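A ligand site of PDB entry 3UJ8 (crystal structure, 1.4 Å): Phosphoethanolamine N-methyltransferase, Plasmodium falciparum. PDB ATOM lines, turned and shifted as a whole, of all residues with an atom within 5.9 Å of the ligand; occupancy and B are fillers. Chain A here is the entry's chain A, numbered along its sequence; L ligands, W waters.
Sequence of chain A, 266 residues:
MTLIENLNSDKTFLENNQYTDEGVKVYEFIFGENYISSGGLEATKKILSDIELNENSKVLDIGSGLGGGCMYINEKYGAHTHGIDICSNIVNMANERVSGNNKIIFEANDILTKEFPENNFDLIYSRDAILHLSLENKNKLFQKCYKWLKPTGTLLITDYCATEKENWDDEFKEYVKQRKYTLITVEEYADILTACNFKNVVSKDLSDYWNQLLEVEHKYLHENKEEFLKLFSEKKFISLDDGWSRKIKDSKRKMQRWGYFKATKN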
ATOM      1  N   LEU A  14      -9.344  -2.127  24.014  1.00  0.00           N
ATOM      2  CA  LEU A  14      -8.905  -1.588  22.725  1.00  0.00           C
ATOM      3  C   LEU A  14      -9.219  -2.525  21.556  1.00  0.00           C
ATOM      4  O   LEU A  14      -9.725  -2.081  20.530  1.00  0.00           O
ATOM      5  CB  LEU A  14      -7.415  -1.261  22.783  1.00  0.00           C
ATOM      6  CG  LEU A  14      -7.089  -0.150  23.781  1.00  0.00           C
ATOM      7  CD1 LEU A  14      -5.585  -0.030  23.958  1.00  0.00           C
ATOM      8  CD2 LEU A  14      -7.688   1.181  23.352  1.00  0.00           C
ATOM      9  N   TYR A  19     -10.196  -0.459  18.216  1.00  0.00           N
ATOM     10  CA  TYR A  19      -9.281  -1.088  17.267  1.00  0.00           C
ATOM     11  C   TYR A  19      -9.673  -2.526  16.921  1.00  0.00           C
ATOM     12  O   TYR A  19      -8.822  -3.415  16.839  1.00  0.00           O
ATOM     13  CB  TYR A  19      -7.841  -1.012  17.783  1.00  0.00           C
ATOM     14  CG  TYR A  19      -7.336   0.411  18.058  1.00  0.00           C
ATOM     15  CD1 TYR A  19      -7.108   1.309  17.029  1.00  0.00           C
ATOM     16  CD2 TYR A  19      -7.095   0.836  19.355  1.00  0.00           C
ATOM     17  CE1 TYR A  19      -6.644   2.590  17.281  1.00  0.00           C
ATOM     18  CE2 TYR A  19      -6.617   2.124  19.625  1.00  0.00           C
ATOM     19  CZ  TYR A  19      -6.407   2.992  18.584  1.00  0.00           C
ATOM     20  OH  TYR A  19      -5.943   4.267  18.827  1.00  0.00           O
ATOM     21  N   ASN A  34      -1.400   1.425   5.586  1.00  0.00           N
ATOM     22  CA  ASN A  34      -0.449   1.158   6.661  1.00  0.00           C
ATOM     23  C   ASN A  34      -0.474   2.163   7.819  1.00  0.00           C
ATOM     24  O   ASN A  34       0.308   2.041   8.771  1.00  0.00           O
ATOM     25  CB  ASN A  34       0.978   1.035   6.122  1.00  0.00           C
ATOM     26  CG  ASN A  34       1.115  -0.075   5.096  1.00  0.00           C
ATOM     27  OD1 ASN A  34       0.503  -1.131   5.226  1.00  0.00           O
ATOM     28  ND2 ASN A  34       1.930   0.161   4.074  1.00  0.00           N
ATOM     29  N   TYR A  35      -1.360   3.158   7.735  1.00  0.00           N
ATOM     30  CA  TYR A  35      -1.464   4.177   8.782  1.00  0.00           C
ATOM     31  C   TYR A  35      -2.859   4.205   9.386  1.00  0.00           C
ATOM     32  O   TYR A  35      -3.863   4.029   8.681  1.00  0.00           O
ATOM     33  CB  TYR A  35      -1.120   5.557   8.232  1.00  0.00           C
ATOM     34  CG  TYR A  35       0.343   5.695   7.903  1.00  0.00           C
ATOM     35  CD1 TYR A  35       0.820   5.408   6.632  1.00  0.00           C
ATOM     36  CD2 TYR A  35       1.246   6.098   8.868  1.00  0.00           C
ATOM     37  CE1 TYR A  35       2.169   5.531   6.335  1.00  0.00           C
ATOM     38  CE2 TYR A  35       2.589   6.217   8.587  1.00  0.00           C
ATOM     39  CZ  TYR A  35       3.044   5.940   7.323  1.00  0.00           C
ATOM     40  OH  TYR A  35       4.377   6.064   7.051  1.00  0.00           O
ATOM     41  N   ILE A  36      -2.921   4.434  10.694  1.00  0.00           N
ATOM     42  CA  ILE A  36      -4.197   4.625  11.363  1.00  0.00           C
ATOM     43  C   ILE A  36      -4.169   5.859  12.251  1.00  0.00           C
ATOM     44  O   ILE A  36      -4.910   5.943  13.225  1.00  0.00           O
ATOM     45  CB  ILE A  36      -4.678   3.360  12.152  1.00  0.00           C
ATOM     46  CG1 ILE A  36      -3.714   2.981  13.280  1.00  0.00           C
ATOM     47  CG2 ILE A  36      -4.871   2.195  11.191  1.00  0.00           C
ATOM     48  CD1 ILE A  36      -4.247   1.839  14.178  1.00  0.00           C
ATOM     49  N   SER A  37      -3.344   6.835  11.877  1.00  0.00           N
ATOM     50  CA  SER A  37      -3.303   8.096  12.611  1.00  0.00           C
ATOM     51  C   SER A  37      -3.064   9.305  11.714  1.00  0.00           C
ATOM     52  O   SER A  37      -2.624   9.171  10.552  1.00  0.00           O
ATOM     53  CB  SER A  37      -2.223   8.057  13.711  1.00  0.00           C
ATOM     54  OG  SER A  37      -0.931   8.224  13.147  1.00  0.00           O
ATOM     55  N   SER A  38      -3.311  10.467  12.275  1.00  0.00           N
ATOM     56  CA  SER A  38      -3.210  11.778  11.651  1.00  0.00           C
ATOM     57  C   SER A  38      -2.198  11.915  10.531  1.00  0.00           C
ATOM     58  O   SER A  38      -1.054  11.757  10.725  1.00  0.00           O
ATOM     59  CB  SER A  38      -2.814  12.782  12.734  1.00  0.00           C
ATOM     60  OG  SER A  38      -3.593  12.653  13.873  1.00  0.00           O
ATOM     61  N   ASP A  61       9.137   1.922  18.059  1.00  0.00           N
ATOM     62  CA  ASP A  61       7.892   2.615  17.779  1.00  0.00           C
ATOM     63  C   ASP A  61       6.862   2.140  18.803  1.00  0.00           C
ATOM     64  O   ASP A  61       6.470   0.972  18.792  1.00  0.00           O
ATOM     65  CB  ASP A  61       7.422   2.305  16.349  1.00  0.00           C
ATOM     66  CG  ASP A  61       6.163   3.058  15.968  1.00  0.00           C
ATOM     67  OD1 ASP A  61       5.455   3.539  16.871  1.00  0.00           O
ATOM     68  OD2 ASP A  61       5.851   3.165  14.767  1.00  0.00           O
ATOM     69  N   ILE A  62       6.455   3.041  19.693  1.00  0.00           N
ATOM     70  CA  ILE A  62       5.518   2.722  20.752  1.00  0.00           C
ATOM     71  C   ILE A  62       4.101   2.922  20.253  1.00  0.00           C
ATOM     72  O   ILE A  62       3.668   4.052  19.980  1.00  0.00           O
ATOM     73  CB  ILE A  62       5.748   3.591  22.007  1.00  0.00           C
ATOM     74  CG1 ILE A  62       7.126   3.310  22.588  1.00  0.00           C
ATOM     75  CG2 ILE A  62       4.646   3.322  23.021  1.00  0.00           C
ATOM     76  CD1 ILE A  62       7.556   4.298  23.668  1.00  0.00           C
ATOM     77  N   GLY A  63       3.369   1.812  20.122  1.00  0.00           N
ATOM     78  CA  GLY A  63       2.023   1.819  19.584  1.00  0.00           C
ATOM     79  C   GLY A  63       2.074   1.793  18.070  1.00  0.00           C
ATOM     80  O   GLY A  63       1.530   2.671  17.401  1.00  0.00           O
ATOM     81  N   SER A  64       2.752   0.788  17.524  1.00  0.00           N
ATOM     82  CA  SER A  64       3.154   0.786  16.112  1.00  0.00           C
ATOM     83  C   SER A  64       2.037   0.565  15.087  1.00  0.00           C
ATOM     84  O   SER A  64       2.235   0.785  13.893  1.00  0.00           O
ATOM     85  CB  SER A  64       4.296  -0.196  15.897  1.00  0.00           C
ATOM     86  OG  SER A  64       3.971  -1.470  16.437  1.00  0.00           O
ATOM     87  N   GLY A  65       0.864   0.142  15.544  1.00  0.00           N
ATOM     88  CA  GLY A  65      -0.289   0.043  14.653  1.00  0.00           C
ATOM     89  C   GLY A  65      -0.091  -0.933  13.501  1.00  0.00           C
ATOM     90  O   GLY A  65       0.386  -2.054  13.699  1.00  0.00           O
ATOM     91  N   LEU A  66      -0.466  -0.504  12.298  1.00  0.00           N
ATOM     92  CA  LEU A  66      -0.302  -1.345  11.113  1.00  0.00           C
ATOM     93  C   LEU A  66       1.119  -1.319  10.580  1.00  0.00           C
ATOM     94  O   LEU A  66       1.434  -2.001   9.606  1.00  0.00           O
ATOM     95  CB  LEU A  66      -1.254  -0.887  10.010  1.00  0.00           C
ATOM     96  CG  LEU A  66      -2.737  -1.172  10.266  1.00  0.00           C
ATOM     97  CD1 LEU A  66      -3.570  -0.630   9.114  1.00  0.00           C
ATOM     98  CD2 LEU A  66      -2.957  -2.664  10.422  1.00  0.00           C
ATOM     99  N   ILE A  84       6.022  -2.006  18.930  1.00  0.00           N
ATOM    100  CA  ILE A  84       5.260  -2.656  19.980  1.00  0.00           C
ATOM    101  C   ILE A  84       3.835  -2.135  19.917  1.00  0.00           C
ATOM    102  O   ILE A  84       3.599  -0.912  19.868  1.00  0.00           O
ATOM    103  CB  ILE A  84       5.845  -2.337  21.370  1.00  0.00           C
ATOM    104  CG1 ILE A  84       7.255  -2.906  21.512  1.00  0.00           C
ATOM    105  CG2 ILE A  84       4.928  -2.894  22.456  1.00  0.00           C
ATOM    106  CD1 ILE A  84       7.289  -4.393  21.740  1.00  0.00           C
ATOM    107  N   ASP A  85       2.863  -3.040  19.917  1.00  0.00           N
ATOM    108  CA  ASP A  85       1.463  -2.630  19.970  1.00  0.00           C
ATOM    109  C   ASP A  85       0.696  -3.613  20.841  1.00  0.00           C
ATOM    110  O   ASP A  85       0.912  -4.824  20.765  1.00  0.00           O
ATOM    111  CB  ASP A  85       0.855  -2.563  18.573  1.00  0.00           C
ATOM    112  CG  ASP A  85      -0.405  -1.729  18.542  1.00  0.00           C
ATOM    113  OD1 ASP A  85      -1.439  -2.209  19.064  1.00  0.00           O
ATOM    114  OD2 ASP A  85      -0.371  -0.600  18.021  1.00  0.00           O
ATOM    115  N   ILE A  86      -0.189  -3.103  21.678  1.00  0.00           N
ATOM    116  CA  ILE A  86      -0.880  -3.946  22.637  1.00  0.00           C
ATOM    117  C   ILE A  86      -1.968  -4.815  21.990  1.00  0.00           C
ATOM    118  O   ILE A  86      -2.317  -5.867  22.517  1.00  0.00           O
ATOM    119  CB  ILE A  86      -1.472  -3.093  23.784  1.00  0.00           C
ATOM    120  CG1 ILE A  86      -1.898  -3.971  24.977  1.00  0.00           C
ATOM    121  CG2 ILE A  86      -2.622  -2.215  23.294  1.00  0.00           C
ATOM    122  CD1 ILE A  86      -2.232  -3.159  26.221  1.00  0.00           C
ATOM    123  N   CYS A  87      -2.478  -4.379  20.840  1.00  0.00           N
ATOM    124  CA  CYS A  87      -3.573  -5.103  20.191  1.00  0.00           C
ATOM    125  C   CYS A  87      -3.014  -6.215  19.286  1.00  0.00           C
ATOM    126  O   CYS A  87      -2.394  -5.952  18.253  1.00  0.00           O
ATOM    127  CB  CYS A  87      -4.444  -4.134  19.388  1.00  0.00           C
ATOM    128  SG  CYS A  87      -5.452  -3.071  20.438  1.00  0.00           S
ATOM    129  N   ILE A  90      -4.065  -6.176  15.586  1.00  0.00           N
ATOM    130  CA  ILE A  90      -3.376  -5.180  14.801  1.00  0.00           C
ATOM    131  C   ILE A  90      -1.972  -5.645  14.428  1.00  0.00           C
ATOM    132  O   ILE A  90      -1.522  -5.470  13.296  1.00  0.00           O
ATOM    133  CB  ILE A  90      -3.279  -3.848  15.564  1.00  0.00           C
ATOM    134  CG1 ILE A  90      -4.651  -3.206  15.710  1.00  0.00           C
ATOM    135  CG2 ILE A  90      -2.334  -2.886  14.869  1.00  0.00           C
ATOM    136  CD1 ILE A  90      -4.579  -1.858  16.422  1.00  0.00           C
ATOM    137  N   ASN A 109       2.454  -6.515  22.671  1.00  0.00           N
ATOM    138  CA  ASN A 109       2.740  -6.406  24.085  1.00  0.00           C
ATOM    139  C   ASN A 109       2.295  -5.046  24.583  1.00  0.00           C
ATOM    140  O   ASN A 109       2.173  -4.106  23.800  1.00  0.00           O
ATOM    141  CB  ASN A 109       4.235  -6.547  24.322  1.00  0.00           C
ATOM    142  CG  ASN A 109       4.566  -7.382  25.539  1.00  0.00           C
ATOM    143  OD1 ASN A 109       4.327  -6.973  26.669  1.00  0.00           O
ATOM    144  ND2 ASN A 109       5.138  -8.565  25.302  1.00  0.00           N
ATOM    145  N   ASP A 110       2.028  -4.951  25.884  1.00  0.00           N
ATOM    146  CA  ASP A 110       1.803  -3.682  26.549  1.00  0.00           C
ATOM    147  C   ASP A 110       3.167  -3.018  26.752  1.00  0.00           C
ATOM    148  O   ASP A 110       4.066  -3.611  27.347  1.00  0.00           O
ATOM    149  CB  ASP A 110       1.157  -3.938  27.903  1.00  0.00           C
ATOM    150  CG  ASP A 110       0.714  -2.675  28.611  1.00  0.00           C
ATOM    151  OD1 ASP A 110       1.154  -1.564  28.265  1.00  0.00           O
ATOM    152  OD2 ASP A 110      -0.080  -2.828  29.563  1.00  0.00           O
ATOM    153  N   ILE A 111       3.336  -1.804  26.258  1.00  0.00           N
ATOM    154  CA  ILE A 111       4.612  -1.119  26.410  1.00  0.00           C
ATOM    155  C   ILE A 111       4.970  -0.928  27.894  1.00  0.00           C
ATOM    156  O   ILE A 111       6.156  -0.852  28.243  1.00  0.00           O
ATOM    157  CB  ILE A 111       4.645   0.220  25.638  1.00  0.00           C
ATOM    158  CG1 ILE A 111       6.087   0.752  25.557  1.00  0.00           C
ATOM    159  CG2 ILE A 111       3.721   1.253  26.280  1.00  0.00           C
ATOM    160  CD1 ILE A 111       7.050  -0.132  24.750  1.00  0.00           C
ATOM    161  N   LEU A 112       3.967  -0.910  28.755  1.00  0.00           N
ATOM    162  CA  LEU A 112       4.201  -0.675  30.184  1.00  0.00           C
ATOM    163  C   LEU A 112       4.807  -1.867  30.914  1.00  0.00           C
ATOM    164  O   LEU A 112       5.360  -1.712  32.014  1.00  0.00           O
ATOM    165  CB  LEU A 112       2.905  -0.244  30.878  1.00  0.00           C
ATOM    166  CG  LEU A 112       2.332   1.099  30.436  1.00  0.00           C
ATOM    167  CD1 LEU A 112       0.923   1.271  30.960  1.00  0.00           C
ATOM    168  CD2 LEU A 112       3.220   2.246  30.891  1.00  0.00           C
ATOM    169  N   SER A 126       6.762   7.721  18.779  1.00  0.00           N
ATOM    170  CA  SER A 126       5.386   7.356  19.070  1.00  0.00           C
ATOM    171  C   SER A 126       4.441   8.351  18.432  1.00  0.00           C
ATOM    172  O   SER A 126       4.630   9.553  18.544  1.00  0.00           O
ATOM    173  CB  SER A 126       5.154   7.281  20.575  1.00  0.00           C
ATOM    174  OG  SER A 126       3.845   6.776  20.860  1.00  0.00           O
ATOM    175  N   ARG A 127       3.413   7.837  17.748  1.00  0.00           N
ATOM    176  CA  ARG A 127       2.454   8.658  17.033  1.00  0.00           C
ATOM    177  C   ARG A 127       1.023   8.367  17.474  1.00  0.00           C
ATOM    178  O   ARG A 127       0.480   7.306  17.150  1.00  0.00           O
ATOM    179  CB  ARG A 127       2.597   8.424  15.517  1.00  0.00           C
ATOM    180  CG  ARG A 127       4.024   8.727  14.976  1.00  0.00           C
ATOM    181  CD  ARG A 127       4.336  10.237  14.969  1.00  0.00           C
ATOM    182  NE  ARG A 127       3.279  10.953  14.283  1.00  0.00           N
ATOM    183  CZ  ARG A 127       3.149  11.003  12.962  1.00  0.00           C
ATOM    184  NH1 ARG A 127       4.048  10.418  12.173  1.00  0.00           N
ATOM    185  NH2 ARG A 127       2.123  11.650  12.409  1.00  0.00           N
ATOM    186  N   ASP A 128       0.458   9.294  18.235  1.00  0.00           N
ATOM    187  CA  ASP A 128      -0.942   9.249  18.652  1.00  0.00           C
ATOM    188  C   ASP A 128      -1.309   7.948  19.359  1.00  0.00           C
ATOM    189  O   ASP A 128      -2.319   7.326  19.049  1.00  0.00           O
ATOM    190  CB  ASP A 128      -1.892   9.557  17.478  1.00  0.00           C
ATOM    191  CG  ASP A 128      -1.625  10.919  16.842  1.00  0.00           C
ATOM    192  OD1 ASP A 128      -0.830  11.730  17.386  1.00  0.00           O
ATOM    193  OD2 ASP A 128      -2.241  11.183  15.776  1.00  0.00           O
ATOM    194  N   ALA A 129      -0.485   7.578  20.332  1.00  0.00           N
ATOM    195  CA  ALA A 129      -0.666   6.345  21.089  1.00  0.00           C
ATOM    196  C   ALA A 129      -0.767   6.597  22.575  1.00  0.00           C
ATOM    197  O   ALA A 129      -1.477   5.895  23.288  1.00  0.00           O
ATOM    198  CB  ALA A 129       0.477   5.386  20.803  1.00  0.00           C
ATOM    199  N   LEU A 131      -2.048   8.902  24.329  1.00  0.00           N
ATOM    200  CA  LEU A 131      -3.361   9.340  24.809  1.00  0.00           C
ATOM    201  C   LEU A 131      -4.128   8.219  25.508  1.00  0.00           C
ATOM    202  O   LEU A 131      -5.025   8.479  26.306  1.00  0.00           O
ATOM    203  CB  LEU A 131      -4.201   9.923  23.661  1.00  0.00           C
ATOM    204  CG  LEU A 131      -4.835   8.950  22.658  1.00  0.00           C
ATOM    205  CD1 LEU A 131      -5.833   9.670  21.770  1.00  0.00           C
ATOM    206  CD2 LEU A 131      -3.772   8.261  21.816  1.00  0.00           C
ATOM    207  N   HIS A 132      -3.802   6.970  25.184  1.00  0.00           N
ATOM    208  CA  HIS A 132      -4.473   5.826  25.779  1.00  0.00           C
ATOM    209  C   HIS A 132      -4.026   5.562  27.219  1.00  0.00           C
ATOM    210  O   HIS A 132      -4.718   4.839  27.948  1.00  0.00           O
ATOM    211  CB  HIS A 132      -4.230   4.576  24.928  1.00  0.00           C
ATOM    212  CG  HIS A 132      -4.928   4.611  23.615  1.00  0.00           C
ATOM    213  ND1 HIS A 132      -6.301   4.597  23.512  1.00  0.00           N
ATOM    214  CD2 HIS A 132      -4.443   4.657  22.341  1.00  0.00           C
ATOM    215  CE1 HIS A 132      -6.630   4.646  22.230  1.00  0.00           C
ATOM    216  NE2 HIS A 132      -5.532   4.670  21.510  1.00  0.00           N
ATOM    217  N   LEU A 133      -2.901   6.132  27.630  1.00  0.00           N
ATOM    218  CA  LEU A 133      -2.335   5.859  28.940  1.00  0.00           C
ATOM    219  C   LEU A 133      -2.830   6.863  29.996  1.00  0.00           C
ATOM    220  O   LEU A 133      -2.939   8.053  29.733  1.00  0.00           O
ATOM    221  CB  LEU A 133      -0.811   5.926  28.874  1.00  0.00           C
ATOM    222  CG  LEU A 133      -0.084   4.665  28.420  1.00  0.00           C
ATOM    223  CD1 LEU A 133      -0.537   4.208  27.032  1.00  0.00           C
ATOM    224  CD2 LEU A 133       1.414   4.899  28.425  1.00  0.00           C
HETATM  225  N1  LIG L   1       1.234   4.812  15.634  1.00  0.00           N
HETATM  226  C1  LIG L   1       0.320   4.108  14.828  1.00  0.00           C
HETATM  227  C2  LIG L   1      -0.064   5.007  13.666  1.00  0.00           C
HETATM  228  O1  LIG L   1       0.345   6.191  13.623  1.00  0.00           O
HETATM  229  O2  LIG L   1      -0.773   4.559  12.687  1.00  0.00           O
HETATM  230  C3  LIG L   1      -0.908   3.670  15.690  1.00  0.00           C
HETATM  231  C4  LIG L   1      -1.812   4.813  16.278  1.00  0.00           C
HETATM  232  C5  LIG L   1      -2.874   4.390  17.249  1.00  0.00           C
HETATM  233  N2  LIG L   1      -3.792   5.504  17.459  1.00  0.00           N
HETATM  234  C6  LIG L   1      -2.299   3.942  18.586  1.00  0.00           C
HETATM  235  C7  LIG L   1      -1.897   2.571  18.839  1.00  0.00           C
HETATM  236  O3  LIG L   1      -1.409   2.515  20.221  1.00  0.00           O
HETATM  237  C8  LIG L   1      -2.957   1.526  18.739  1.00  0.00           C
HETATM  238  O4  LIG L   1      -2.664   0.693  17.670  1.00  0.00           O
HETATM  239  C9  LIG L   1      -2.975   0.864  20.080  1.00  0.00           C
HETATM  240  O5  LIG L   1      -3.237  -0.506  20.058  1.00  0.00           O
HETATM  241  C10 LIG L   1      -1.634   1.218  20.671  1.00  0.00           C
HETATM  242  N3  LIG L   1      -1.576   1.173  22.146  1.00  0.00           N
HETATM  243  C11 LIG L   1      -2.426   1.719  23.030  1.00  0.00           C
HETATM  244  N4  LIG L   1      -1.971   1.451  24.264  1.00  0.00           N
HETATM  245  C12 LIG L   1      -0.827   0.745  24.158  1.00  0.00           C
HETATM  246  C13 LIG L   1       0.055   0.200  25.103  1.00  0.00           C
HETATM  247  N5  LIG L   1      -0.176   0.311  26.440  1.00  0.00           N
HETATM  248  N6  LIG L   1       1.129  -0.477  24.652  1.00  0.00           N
HETATM  249  C14 LIG L   1       1.338  -0.622  23.331  1.00  0.00           C
HETATM  250  N7  LIG L   1       0.519  -0.126  22.397  1.00  0.00           N
HETATM  251  C15 LIG L   1      -0.570   0.563  22.787  1.00  0.00           C
HETATM  252  O   HOH W   1      -4.913   7.127  15.558  1.00  0.00           O
HETATM  253  O   HOH W   2       1.947   7.729  11.817  1.00  0.00           O
HETATM  254  O   HOH W   3      -0.020   2.266  11.487  1.00  0.00           O
HETATM  255  O   HOH W   4       2.474   3.669  11.793  1.00  0.00           O
HETATM  256  O   HOH W   5       3.662   4.801  14.048  1.00  0.00           O
HETATM  257  O   HOH W   6       3.380   5.072  17.399  1.00  0.00           O
HETATM  258  O   HOH W   7      -3.251   1.409  26.867  1.00  0.00           O
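Merely in contact with the ligand: Ile 90 (3.4 Å), Ala 129 (3.5 Å), Asn 109 (3.6 Å), His 132 (3.6 Å), Leu 14 (3.7 Å), Gly 65 (3.8 Å), Tyr 35 (3.9 Å), Ser 64 (3.9 Å) and Leu 133 (3.96 Å). Hydrophobic or aromatic side chains within 4 Å of the ligand: Leu 14, Tyr 19, Ile 36, Ile 86, Ile 90, Ile 111, Ala 129, His 132 and Leu 133. 20 residues have an atom within 4 Å of the ligand: Leu 14, Tyr 19, Tyr 35, Ile 36, Ser 37, Gly 63, Ser 64, Gly 65, Asp 85, Ile 86, Cys 87, Ile 90, Asn 109, Asp 110, Ile 111, Arg 127, Asp 128, Ala 129, His 132 and Leu 133.
The backbone NH of Gly 63 is in hydrogen-bond range of the backbone carbonyl oxygen of Ile 84 (2.7 Å). The side-chain carboxylate (OD2) of Asp 128 is in hydrogen-bond range of the side-chain hydroxyl (OG) of Ser 38, 2.8 Å away. The backbone carbonyl oxygen (O) of Leu 14 lies within hydrogen-bond range of the backbone NH (N) of Tyr 19. The side-chain hydroxyl of Tyr 19 sits at hydrogen-bond distance from a ring nitrogen (NE2) of His 132. OD1 of Asp 110 is in hydrogen-bond range of N of Leu 112 (2.9 Å). The backbone NH (N) of Gly 65 sits at hydrogen-bond distance from the side-chain carboxylate (OD2) of Asp 85 (2.9 Å). The backbone carbonyl oxygen of Asn 109 lies close to the backbone NH of Ile 86, at 3.3 Å. The side-chain carboxylate (OD1) of Asp 85 lies within hydrogen-bond range of the backbone NH (N) of Cys 87 (3.0 Å).
Water W3 lies within hydrogen-bond range of an oxygen (O2) of the ligand (2.7 Å), the backbone carbonyl oxygen (O) of Asn 34 (2.7 Å) and the backbone NH (N) of Leu 66 (2.9 Å). Water W1 bridges O of Ile 36 and N2 of the ligand. Water W2 lies within hydrogen-bond range of O1 of the ligand, OG of Ser 37 and NH1 of Arg 127. Water W5 bridges OD2 of Asp 61 (2.8 Å) and N1 of the ligand (2.9 Å).
A nitrogen (N7) of the ligand sits at hydrogen-bond distance from the backbone NH of Ile 86 (3.1 Å). The side-chain hydroxyl of Tyr 19 lies within hydrogen-bond range of a nitrogen (N2) of the ligand (2.8 Å). OD1 of Asp 110 sits at hydrogen-bond distance from N5 of the ligand, 2.9 Å away. N2 of the ligand is in hydrogen-bond range of O of Asp 128. OG of Ser 37 is in hydrogen-bond range of O1 of the ligand (2.4 Å). O of Gly 63 is in hydrogen-bond range of N1 of the ligand. N of Ile 36 is in hydrogen-bond range of O2 of the ligand (2.9 Å). N of Ile 111 lies within hydrogen-bond range of N6 of the ligand. The backbone carbonyl oxygen (O) of Arg 127 is in hydrogen-bond range of a nitrogen (N1) of the ligand (3.0 Å). OD2 of Asp 85 lies within hydrogen-bond range of O4 of the ligand, at 2.7 Å. An oxygen (O5) of the ligand is in hydrogen-bond range of the side-chain sulfur of Cys 87, 3.4 Å away.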
